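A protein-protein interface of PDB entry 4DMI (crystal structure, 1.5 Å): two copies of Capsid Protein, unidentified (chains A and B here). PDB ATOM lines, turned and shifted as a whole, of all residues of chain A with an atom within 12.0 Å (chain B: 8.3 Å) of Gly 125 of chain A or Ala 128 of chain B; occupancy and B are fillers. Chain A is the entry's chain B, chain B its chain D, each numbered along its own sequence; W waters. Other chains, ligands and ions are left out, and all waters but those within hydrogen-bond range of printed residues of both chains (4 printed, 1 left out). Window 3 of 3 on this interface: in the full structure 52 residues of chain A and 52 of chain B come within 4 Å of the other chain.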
ATOM      1  N   ASP A  95       1.055  17.686 -26.708  1.00  0.00           N
ATOM      2  CA  ASP A  95       0.221  16.672 -26.063  1.00  0.00           C
ATOM      3  C   ASP A  95      -0.067  15.530 -27.032  1.00  0.00           C
ATOM      4  O   ASP A  95      -0.187  15.746 -28.231  1.00  0.00           O
ATOM      5  CB  ASP A  95      -1.099  17.325 -25.642  1.00  0.00           C
ATOM      6  CG  ASP A  95      -1.955  16.436 -24.764  1.00  0.00           C
ATOM      7  OD1 ASP A  95      -2.157  15.247 -25.091  1.00  0.00           O
ATOM      8  OD2 ASP A  95      -2.449  16.946 -23.738  1.00  0.00           O
ATOM      9  N   GLU A  96      -0.190  14.314 -26.511  1.00  0.00           N
ATOM     10  CA  GLU A  96      -0.467  13.162 -27.369  1.00  0.00           C
ATOM     11  C   GLU A  96      -1.806  13.273 -28.103  1.00  0.00           C
ATOM     12  O   GLU A  96      -1.983  12.667 -29.163  1.00  0.00           O
ATOM     13  CB  GLU A  96      -0.365  11.849 -26.588  1.00  0.00           C
ATOM     14  CG  GLU A  96      -1.326  11.727 -25.427  1.00  0.00           C
ATOM     15  CD  GLU A  96      -2.705  11.238 -25.840  1.00  0.00           C
ATOM     16  OE1 GLU A  96      -3.685  11.521 -25.113  1.00  0.00           O
ATOM     17  OE2 GLU A  96      -2.820  10.570 -26.897  1.00  0.00           O
ATOM     18  N   VAL A 121       3.537  14.147 -25.081  1.00  0.00           N
ATOM     19  CA  VAL A 121       3.375  14.477 -23.662  1.00  0.00           C
ATOM     20  C   VAL A 121       1.960  14.207 -23.141  1.00  0.00           C
ATOM     21  O   VAL A 121       0.985  14.256 -23.888  1.00  0.00           O
ATOM     22  CB  VAL A 121       3.900  15.891 -23.266  1.00  0.00           C
ATOM     23  CG1 VAL A 121       5.263  16.175 -23.906  1.00  0.00           C
ATOM     24  CG2 VAL A 121       2.919  16.962 -23.620  1.00  0.00           C
ATOM     25  N   SER A 122       1.875  13.884 -21.855  1.00  0.00           N
ATOM     26  CA  SER A 122       0.617  13.510 -21.220  1.00  0.00           C
ATOM     27  C   SER A 122       0.434  14.296 -19.930  1.00  0.00           C
ATOM     28  O   SER A 122       0.664  13.772 -18.833  1.00  0.00           O
ATOM     29  CB  SER A 122       0.624  12.022 -20.884  1.00  0.00           C
ATOM     30  OG  SER A 122      -0.648  11.617 -20.412  1.00  0.00           O
ATOM     31  N   PRO A 123       0.022  15.561 -20.047  1.00  0.00           N
ATOM     32  CA  PRO A 123      -0.163  16.400 -18.855  1.00  0.00           C
ATOM     33  C   PRO A 123      -1.343  15.919 -18.009  1.00  0.00           C
ATOM     34  O   PRO A 123      -2.258  15.280 -18.532  1.00  0.00           O
ATOM     35  CB  PRO A 123      -0.467  17.775 -19.450  1.00  0.00           C
ATOM     36  CG  PRO A 123      -1.119  17.468 -20.783  1.00  0.00           C
ATOM     37  CD  PRO A 123      -0.383  16.245 -21.287  1.00  0.00           C
ATOM     38  N   ASP A 124      -1.310  16.201 -16.712  1.00  0.00           N
ATOM     39  CA  ASP A 124      -2.435  15.863 -15.857  1.00  0.00           C
ATOM     40  C   ASP A 124      -2.736  17.027 -14.931  1.00  0.00           C
ATOM     41  O   ASP A 124      -1.819  17.656 -14.411  1.00  0.00           O
ATOM     42  CB  ASP A 124      -2.133  14.609 -15.037  1.00  0.00           C
ATOM     43  CG  ASP A 124      -3.315  14.175 -14.188  1.00  0.00           C
ATOM     44  OD1 ASP A 124      -4.449  14.136 -14.712  1.00  0.00           O
ATOM     45  OD2 ASP A 124      -3.111  13.883 -12.991  1.00  0.00           O
ATOM     46  N   GLY A 125      -4.018  17.315 -14.732  1.00  0.00           N
ATOM     47  CA  GLY A 125      -4.418  18.340 -13.782  1.00  0.00           C
ATOM     48  C   GLY A 125      -4.268  19.760 -14.287  1.00  0.00           C
ATOM     49  O   GLY A 125      -4.289  20.710 -13.506  1.00  0.00           O
ATOM     50  N   THR A 126      -4.121  19.911 -15.597  1.00  0.00           N
ATOM     51  CA  THR A 126      -3.932  21.232 -16.182  1.00  0.00           C
ATOM     52  C   THR A 126      -4.185  21.225 -17.682  1.00  0.00           C
ATOM     53  O   THR A 126      -3.907  20.235 -18.361  1.00  0.00           O
ATOM     54  CB  THR A 126      -2.509  21.777 -15.908  1.00  0.00           C
ATOM     55  OG1 THR A 126      -2.380  23.097 -16.460  1.00  0.00           O
ATOM     56  CG2 THR A 126      -1.455  20.866 -16.517  1.00  0.00           C
ATOM     57  N   THR A 127      -4.724  22.331 -18.190  1.00  0.00           N
ATOM     58  CA  THR A 127      -4.852  22.536 -19.631  1.00  0.00           C
ATOM     59  C   THR A 127      -3.755  23.441 -20.177  1.00  0.00           C
ATOM     60  O   THR A 127      -3.704  23.723 -21.379  1.00  0.00           O
ATOM     61  CB  THR A 127      -6.231  23.116 -20.010  1.00  0.00           C
ATOM     62  OG1 THR A 127      -6.444  24.348 -19.318  1.00  0.00           O
ATOM     63  CG2 THR A 127      -7.338  22.140 -19.649  1.00  0.00           C
ATOM     64  N   ALA A 128      -2.879  23.902 -19.291  1.00  0.00           N
ATOM     65  CA  ALA A 128      -1.724  24.681 -19.704  1.00  0.00           C
ATOM     66  C   ALA A 128      -0.570  23.717 -19.925  1.00  0.00           C
ATOM     67  O   ALA A 128       0.028  23.237 -18.962  1.00  0.00           O
ATOM     68  CB  ALA A 128      -1.365  25.702 -18.637  1.00  0.00           C
ATOM     69  N   VAL A 129      -0.266  23.432 -21.188  1.00  0.00           N
ATOM     70  CA  VAL A 129       0.668  22.366 -21.532  1.00  0.00           C
ATOM     71  C   VAL A 129       2.001  22.912 -22.005  1.00  0.00           C
ATOM     72  O   VAL A 129       2.104  23.447 -23.120  1.00  0.00           O
ATOM     73  CB  VAL A 129       0.088  21.458 -22.628  1.00  0.00           C
ATOM     74  CG1 VAL A 129       0.976  20.232 -22.835  1.00  0.00           C
ATOM     75  CG2 VAL A 129      -1.326  21.034 -22.260  1.00  0.00           C
ATOM     76  N   GLN A 130       3.021  22.769 -21.161  1.00  0.00           N
ATOM     77  CA  GLN A 130       4.362  23.187 -21.537  1.00  0.00           C
ATOM     78  C   GLN A 130       4.947  22.244 -22.563  1.00  0.00           C
ATOM     79  O   GLN A 130       4.609  21.054 -22.605  1.00  0.00           O
ATOM     80  CB  GLN A 130       5.276  23.258 -20.316  1.00  0.00           C
ATOM     81  CG  GLN A 130       4.807  24.257 -19.250  1.00  0.00           C
ATOM     82  CD  GLN A 130       4.841  25.694 -19.739  1.00  0.00           C
ATOM     83  OE1 GLN A 130       5.713  26.074 -20.529  1.00  0.00           O
ATOM     84  NE2 GLN A 130       3.876  26.492 -19.295  1.00  0.00           N
ATOM     85  N   SER A 131       5.828  22.799 -23.390  1.00  0.00           N
ATOM     86  CA  SER A 131       6.475  22.085 -24.471  1.00  0.00           C
ATOM     87  C   SER A 131       7.997  22.163 -24.350  1.00  0.00           C
ATOM     88  O   SER A 131       8.556  23.156 -23.860  1.00  0.00           O
ATOM     89  CB  SER A 131       6.009  22.694 -25.800  1.00  0.00           C
ATOM     90  OG  SER A 131       6.717  22.210 -26.935  1.00  0.00           O
ATOM     91  N   ARG B  94       4.690  10.264 -16.695  1.00  0.00           N
ATOM     92  CA  ARG B  94       3.627  10.517 -15.717  1.00  0.00           C
ATOM     93  C   ARG B  94       4.227  10.543 -14.312  1.00  0.00           C
ATOM     94  O   ARG B  94       5.356  10.086 -14.089  1.00  0.00           O
ATOM     95  CB  ARG B  94       2.526   9.445 -15.792  1.00  0.00           C
ATOM     96  CG  ARG B  94       1.813   9.373 -17.140  1.00  0.00           C
ATOM     97  CD  ARG B  94       0.903  10.571 -17.387  1.00  0.00           C
ATOM     98  NE  ARG B  94      -0.186  10.654 -16.414  1.00  0.00           N
ATOM     99  CZ  ARG B  94      -1.468  10.849 -16.724  1.00  0.00           C
ATOM    100  NH1 ARG B  94      -1.846  10.956 -17.996  1.00  0.00           N
ATOM    101  NH2 ARG B  94      -2.382  10.915 -15.759  1.00  0.00           N
ATOM    102  N   ASP B  95       3.456  11.084 -13.376  1.00  0.00           N
ATOM    103  CA  ASP B  95       3.762  11.010 -11.945  1.00  0.00           C
ATOM    104  C   ASP B  95       4.045   9.561 -11.560  1.00  0.00           C
ATOM    105  O   ASP B  95       3.400   8.642 -12.063  1.00  0.00           O
ATOM    106  CB  ASP B  95       2.546  11.545 -11.172  1.00  0.00           C
ATOM    107  CG  ASP B  95       2.844  11.883  -9.716  1.00  0.00           C
ATOM    108  OD1 ASP B  95       3.516  11.103  -9.012  1.00  0.00           O
ATOM    109  OD2 ASP B  95       2.369  12.946  -9.269  1.00  0.00           O
ATOM    110  N   PRO B 123       6.255  15.570  -8.805  1.00  0.00           N
ATOM    111  CA  PRO B 123       5.972  16.996  -8.607  1.00  0.00           C
ATOM    112  C   PRO B 123       5.754  17.307  -7.129  1.00  0.00           C
ATOM    113  O   PRO B 123       5.393  16.423  -6.347  1.00  0.00           O
ATOM    114  CB  PRO B 123       4.679  17.208  -9.406  1.00  0.00           C
ATOM    115  CG  PRO B 123       4.000  15.857  -9.389  1.00  0.00           C
ATOM    116  CD  PRO B 123       5.120  14.846  -9.416  1.00  0.00           C
ATOM    117  N   ASP B 124       5.978  18.556  -6.734  1.00  0.00           N
ATOM    118  CA  ASP B 124       5.721  18.945  -5.355  1.00  0.00           C
ATOM    119  C   ASP B 124       4.992  20.271  -5.329  1.00  0.00           C
ATOM    120  O   ASP B 124       5.315  21.172  -6.102  1.00  0.00           O
ATOM    121  CB  ASP B 124       7.030  19.060  -4.577  1.00  0.00           C
ATOM    122  CG  ASP B 124       6.806  19.346  -3.097  1.00  0.00           C
ATOM    123  OD1 ASP B 124       5.957  18.663  -2.474  1.00  0.00           O
ATOM    124  OD2 ASP B 124       7.473  20.259  -2.561  1.00  0.00           O
ATOM    125  N   GLY B 125       4.011  20.397  -4.441  1.00  0.00           N
ATOM    126  CA  GLY B 125       3.313  21.659  -4.279  1.00  0.00           C
ATOM    127  C   GLY B 125       2.364  21.995  -5.412  1.00  0.00           C
ATOM    128  O   GLY B 125       1.981  23.158  -5.584  1.00  0.00           O
ATOM    129  N   THR B 126       1.969  20.984  -6.180  1.00  0.00           N
ATOM    130  CA  THR B 126       1.019  21.198  -7.270  1.00  0.00           C
ATOM    131  C   THR B 126       0.365  19.909  -7.737  1.00  0.00           C
ATOM    132  O   THR B 126       0.962  18.832  -7.657  1.00  0.00           O
ATOM    133  CB  THR B 126       1.687  21.889  -8.483  1.00  0.00           C
ATOM    134  OG1 THR B 126       0.711  22.133  -9.505  1.00  0.00           O
ATOM    135  CG2 THR B 126       2.816  21.038  -9.045  1.00  0.00           C
ATOM    136  N   THR B 127      -0.872  20.029  -8.211  1.00  0.00           N
ATOM    137  CA  THR B 127      -1.563  18.922  -8.866  1.00  0.00           C
ATOM    138  C   THR B 127      -1.589  19.113 -10.378  1.00  0.00           C
ATOM    139  O   THR B 127      -2.171  18.308 -11.110  1.00  0.00           O
ATOM    140  CB  THR B 127      -3.004  18.759  -8.348  1.00  0.00           C
ATOM    141  OG1 THR B 127      -3.738  19.965  -8.582  1.00  0.00           O
ATOM    142  CG2 THR B 127      -2.999  18.445  -6.867  1.00  0.00           C
ATOM    143  N   ALA B 128      -0.961  20.189 -10.844  1.00  0.00           N
ATOM    144  CA  ALA B 128      -0.776  20.399 -12.275  1.00  0.00           C
ATOM    145  C   ALA B 128       0.542  19.767 -12.691  1.00  0.00           C
ATOM    146  O   ALA B 128       1.600  20.384 -12.535  1.00  0.00           O
ATOM    147  CB  ALA B 128      -0.771  21.884 -12.606  1.00  0.00           C
ATOM    148  N   VAL B 129       0.481  18.547 -13.220  1.00  0.00           N
ATOM    149  CA  VAL B 129       1.692  17.775 -13.473  1.00  0.00           C
ATOM    150  C   VAL B 129       2.080  17.793 -14.953  1.00  0.00           C
ATOM    151  O   VAL B 129       1.466  17.112 -15.784  1.00  0.00           O
ATOM    152  CB  VAL B 129       1.533  16.317 -12.979  1.00  0.00           C
ATOM    153  CG1 VAL B 129       2.852  15.553 -13.105  1.00  0.00           C
ATOM    154  CG2 VAL B 129       1.049  16.294 -11.536  1.00  0.00           C
ATOM    155  N   GLN B 130       3.093  18.588 -15.278  1.00  0.00           N
ATOM    156  CA  GLN B 130       3.619  18.621 -16.632  1.00  0.00           C
ATOM    157  C   GLN B 130       4.313  17.322 -16.979  1.00  0.00           C
ATOM    158  O   GLN B 130       4.867  16.633 -16.115  1.00  0.00           O
ATOM    159  CB  GLN B 130       4.611  19.778 -16.802  1.00  0.00           C
ATOM    160  CG  GLN B 130       3.998  21.150 -16.584  1.00  0.00           C
ATOM    161  CD  GLN B 130       2.948  21.513 -17.609  1.00  0.00           C
ATOM    162  OE1 GLN B 130       3.041  21.129 -18.775  1.00  0.00           O
ATOM    163  NE2 GLN B 130       1.936  22.260 -17.178  1.00  0.00           N
ATOM    164  N   SER B 131       4.298  17.011 -18.265  1.00  0.00           N
ATOM    165  CA  SER B 131       4.843  15.764 -18.769  1.00  0.00           C
ATOM    166  C   SER B 131       5.864  16.071 -19.856  1.00  0.00           C
ATOM    167  O   SER B 131       5.752  17.071 -20.575  1.00  0.00           O
ATOM    168  CB  SER B 131       3.689  14.913 -19.314  1.00  0.00           C
ATOM    169  OG  SER B 131       4.149  13.788 -20.036  1.00  0.00           O
ATOM    170  N   GLU B 156      -4.368   7.927 -22.542  1.00  0.00           N
ATOM    171  CA  GLU B 156      -3.651   9.177 -22.301  1.00  0.00           C
ATOM    172  C   GLU B 156      -2.139   9.074 -22.447  1.00  0.00           C
ATOM    173  O   GLU B 156      -1.467  10.098 -22.506  1.00  0.00           O
ATOM    174  CB  GLU B 156      -3.985   9.734 -20.917  1.00  0.00           C
ATOM    175  CG  GLU B 156      -5.454  10.095 -20.749  1.00  0.00           C
ATOM    176  CD  GLU B 156      -5.820  10.399 -19.311  1.00  0.00           C
ATOM    177  OE1 GLU B 156      -4.923  10.343 -18.441  1.00  0.00           O
ATOM    178  OE2 GLU B 156      -7.008  10.694 -19.055  1.00  0.00           O
HETATM  179  O   HOH W   1      -3.136  15.838 -10.942  1.00  0.00           O
HETATM  180  O   HOH W   2      -4.743  20.646 -10.842  1.00  0.00           O
HETATM  181  O   HOH W   3       1.670  14.213 -16.243  1.00  0.00           O
HETATM  182  O   HOH W   4       6.767  19.477 -21.420  1.00  0.00           O
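The side-chain hydroxyl (OG) of Ser 122 of chain A lies within hydrogen-bond range of the guanidinium group (NH1) of Arg 94 of chain B, 2.8 Å away. N of Ser 122 of chain A is in hydrogen-bond range of OG of Ser 131 of chain B (2.9 Å). The backbone carbonyl oxygen (O) of Glu 156 of chain B lies within hydrogen-bond range of the side-chain hydroxyl (OG) of Ser 122 of chain A (2.7 Å). OD1 of Asp 124 of chain A lies within salt-bridge range of NH2 of Arg 94 of chain B (3.97 Å). O of Asp 124 of chain A sits at hydrogen-bond distance from N of Val 129 of chain B, 2.7 Å away. O of Ala 128 of chain A lies within hydrogen-bond range of NE2 of Gln 130 of chain B, at 2.8 Å. N of Gln 130 of chain A is in hydrogen-bond range of OE1 of Gln 130 of chain B (2.9 Å). The backbone carbonyl oxygen of Asp 124 of chain A sits close to the backbone carbonyl oxygen of Thr 127 of chain B, 3.4 Å away.
N of Glu 96 of chain A is in hydrogen-bond range of O of Val 121 of chain A. N of Ala 128 of chain A lies within hydrogen-bond range of OG1 of Thr 126 of chain A (3.0 Å). NH1 of Arg 94 of chain B lies within salt-bridge range of OE1 of Glu 156 of chain B (3.2 Å). The backbone NH (N) of Ala 128 of chain B sits at hydrogen-bond distance from the side-chain hydroxyl (OG1) of Thr 126 of chain B, at 2.9 Å.
Glu 96 of chain A touches Glu 156 of chain B (CG to O, 3.3 Å). Ser 131 of chain B touches Val 121 of chain A (O to CB, 3.5 Å). O of Val 129 of chain B touches CA of Pro 123 of chain A, at 3.5 Å. Pro 123 of chain A touches Ser 131 of chain B (N to CB, 3.8 Å). Asp 124 of chain A touches Ala 128 of chain B. Thr 127 of chain B touches Gly 125 of chain A (O to CA, 3.5 Å). Ala 128 of chain B touches Gly 125 of chain A. CB of Thr 126 of chain A touches CB of Ala 128 of chain B, 3.7 Å away. NE2 of Gln 130 of chain B touches CG2 of Thr 126 of chain A, at 3.7 Å. OE1 of Gln 130 of chain B touches C of Val 129 of chain A (3.8 Å).
Printed residues of chain B within 4 Å of Val 121 of chain A: Ser 131. Printed residues of chain B within 4 Å of Ser 122 of chain A: Arg 94, Ser 131 and Glu 156. Of chain B, only Arg 94 (3.7 Å), Thr 127 (3.4 Å), Ala 128 (3.6 Å) and Val 129 (2.7 Å) come within 4 Å of Asp 124 of chain A. Of chain B, only Thr 127 (3.5 Å) and Ala 128 (3.7 Å) come within 4 Å of Gly 125 of chain A. Asp 124 of chain B touches none of the printed residues of chain A. Gly 125 of chain B touches none of the printed residues of chain A. Of chain A, only Asp 124 (3.4 Å) and Gly 125 (3.5 Å) come within 4 Å of Thr 127 of chain B. Of chain A, only Asp 124 (3.6 Å), Gly 125 (3.7 Å) and Thr 126 (3.7 Å) come within 4 Å of Ala 128 of chain B. Val 129 of chain B touches just these residues of chain A: Pro 123 (3.5 Å) and Asp 124 (2.7 Å). Of the printed residues of chain A, Ser 131 of chain B touches Val 121, Ser 122 and Pro 123. The nearest residue of chain B that does not touch Gly 125 of chain A is Val 129 of chain B (4.9 Å). The nearest residue of chain A that does not touch Ala 128 of chain B is Ala 128 of chain A (6.5 Å).
Printed residues of chain B that touch a printed residue of chain A: Arg 94, Thr 127, Ala 128, Val 129, Gln 130, Ser 131 and Glu 156. Of the 13 printed residues of chain A, 10 touch a printed residue of chain B. Hydrophobic or aromatic side chains of chain A within 4 Å of the printed part of chain B: Val 121. Along chain A the printed residues that touch a printed residue of chain B span positions 96 to 130. Among the printed residues, Asp or Glu carboxylates within 4 Å of a Lys or Arg side-chain nitrogen of the other chain: Asp 124 of chain A with Arg 94 of chain B (3.97 Å).
Pro 123 of chain A touches Ser 131 of chain B, but with the chains exchanged Ser 131 of chain A does not touch Pro 123 of chain B (15.1 Å). Thr 126 of chain A touches Gln 130 of chain B, but with the chains exchanged Gln 130 of chain A does not touch Thr 126 of chain B (10.8 Å). Ala 128 of chain A touches Gln 130 of chain B, but with the chains exchanged Gln 130 of chain A does not touch Ala 128 of chain B (8.4 Å). Gln 130 of chain B touches its own counterpart, Gln 130 of chain A. Positions printed for both chains: 95, 123, 124, 125, 126, 127, 128, 129, 130 and 131.
Water W2 lies within hydrogen-bond range of the side-chain hydroxyl (OG1) of Thr 127 of chain B (2.6 Å) and the backbone carbonyl oxygen (O) of Gly 125 of chain A (2.7 Å). Water W1 lies within hydrogen-bond range of the backbone carbonyl oxygen (O) of Thr 127 of chain B and the side-chain carboxylate (OD2) of Asp 124 of chain A. Water W4 lies within hydrogen-bond range of the backbone carbonyl oxygen (O) of Ser 131 of chain B (2.7 Å) and the backbone carbonyl oxygen (O) of Gln 130 of chain A (2.9 Å). Water W3 bridges O of Ser 122 of chain A (2.8 Å) and O of Val 129 of chain B (2.9 Å).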
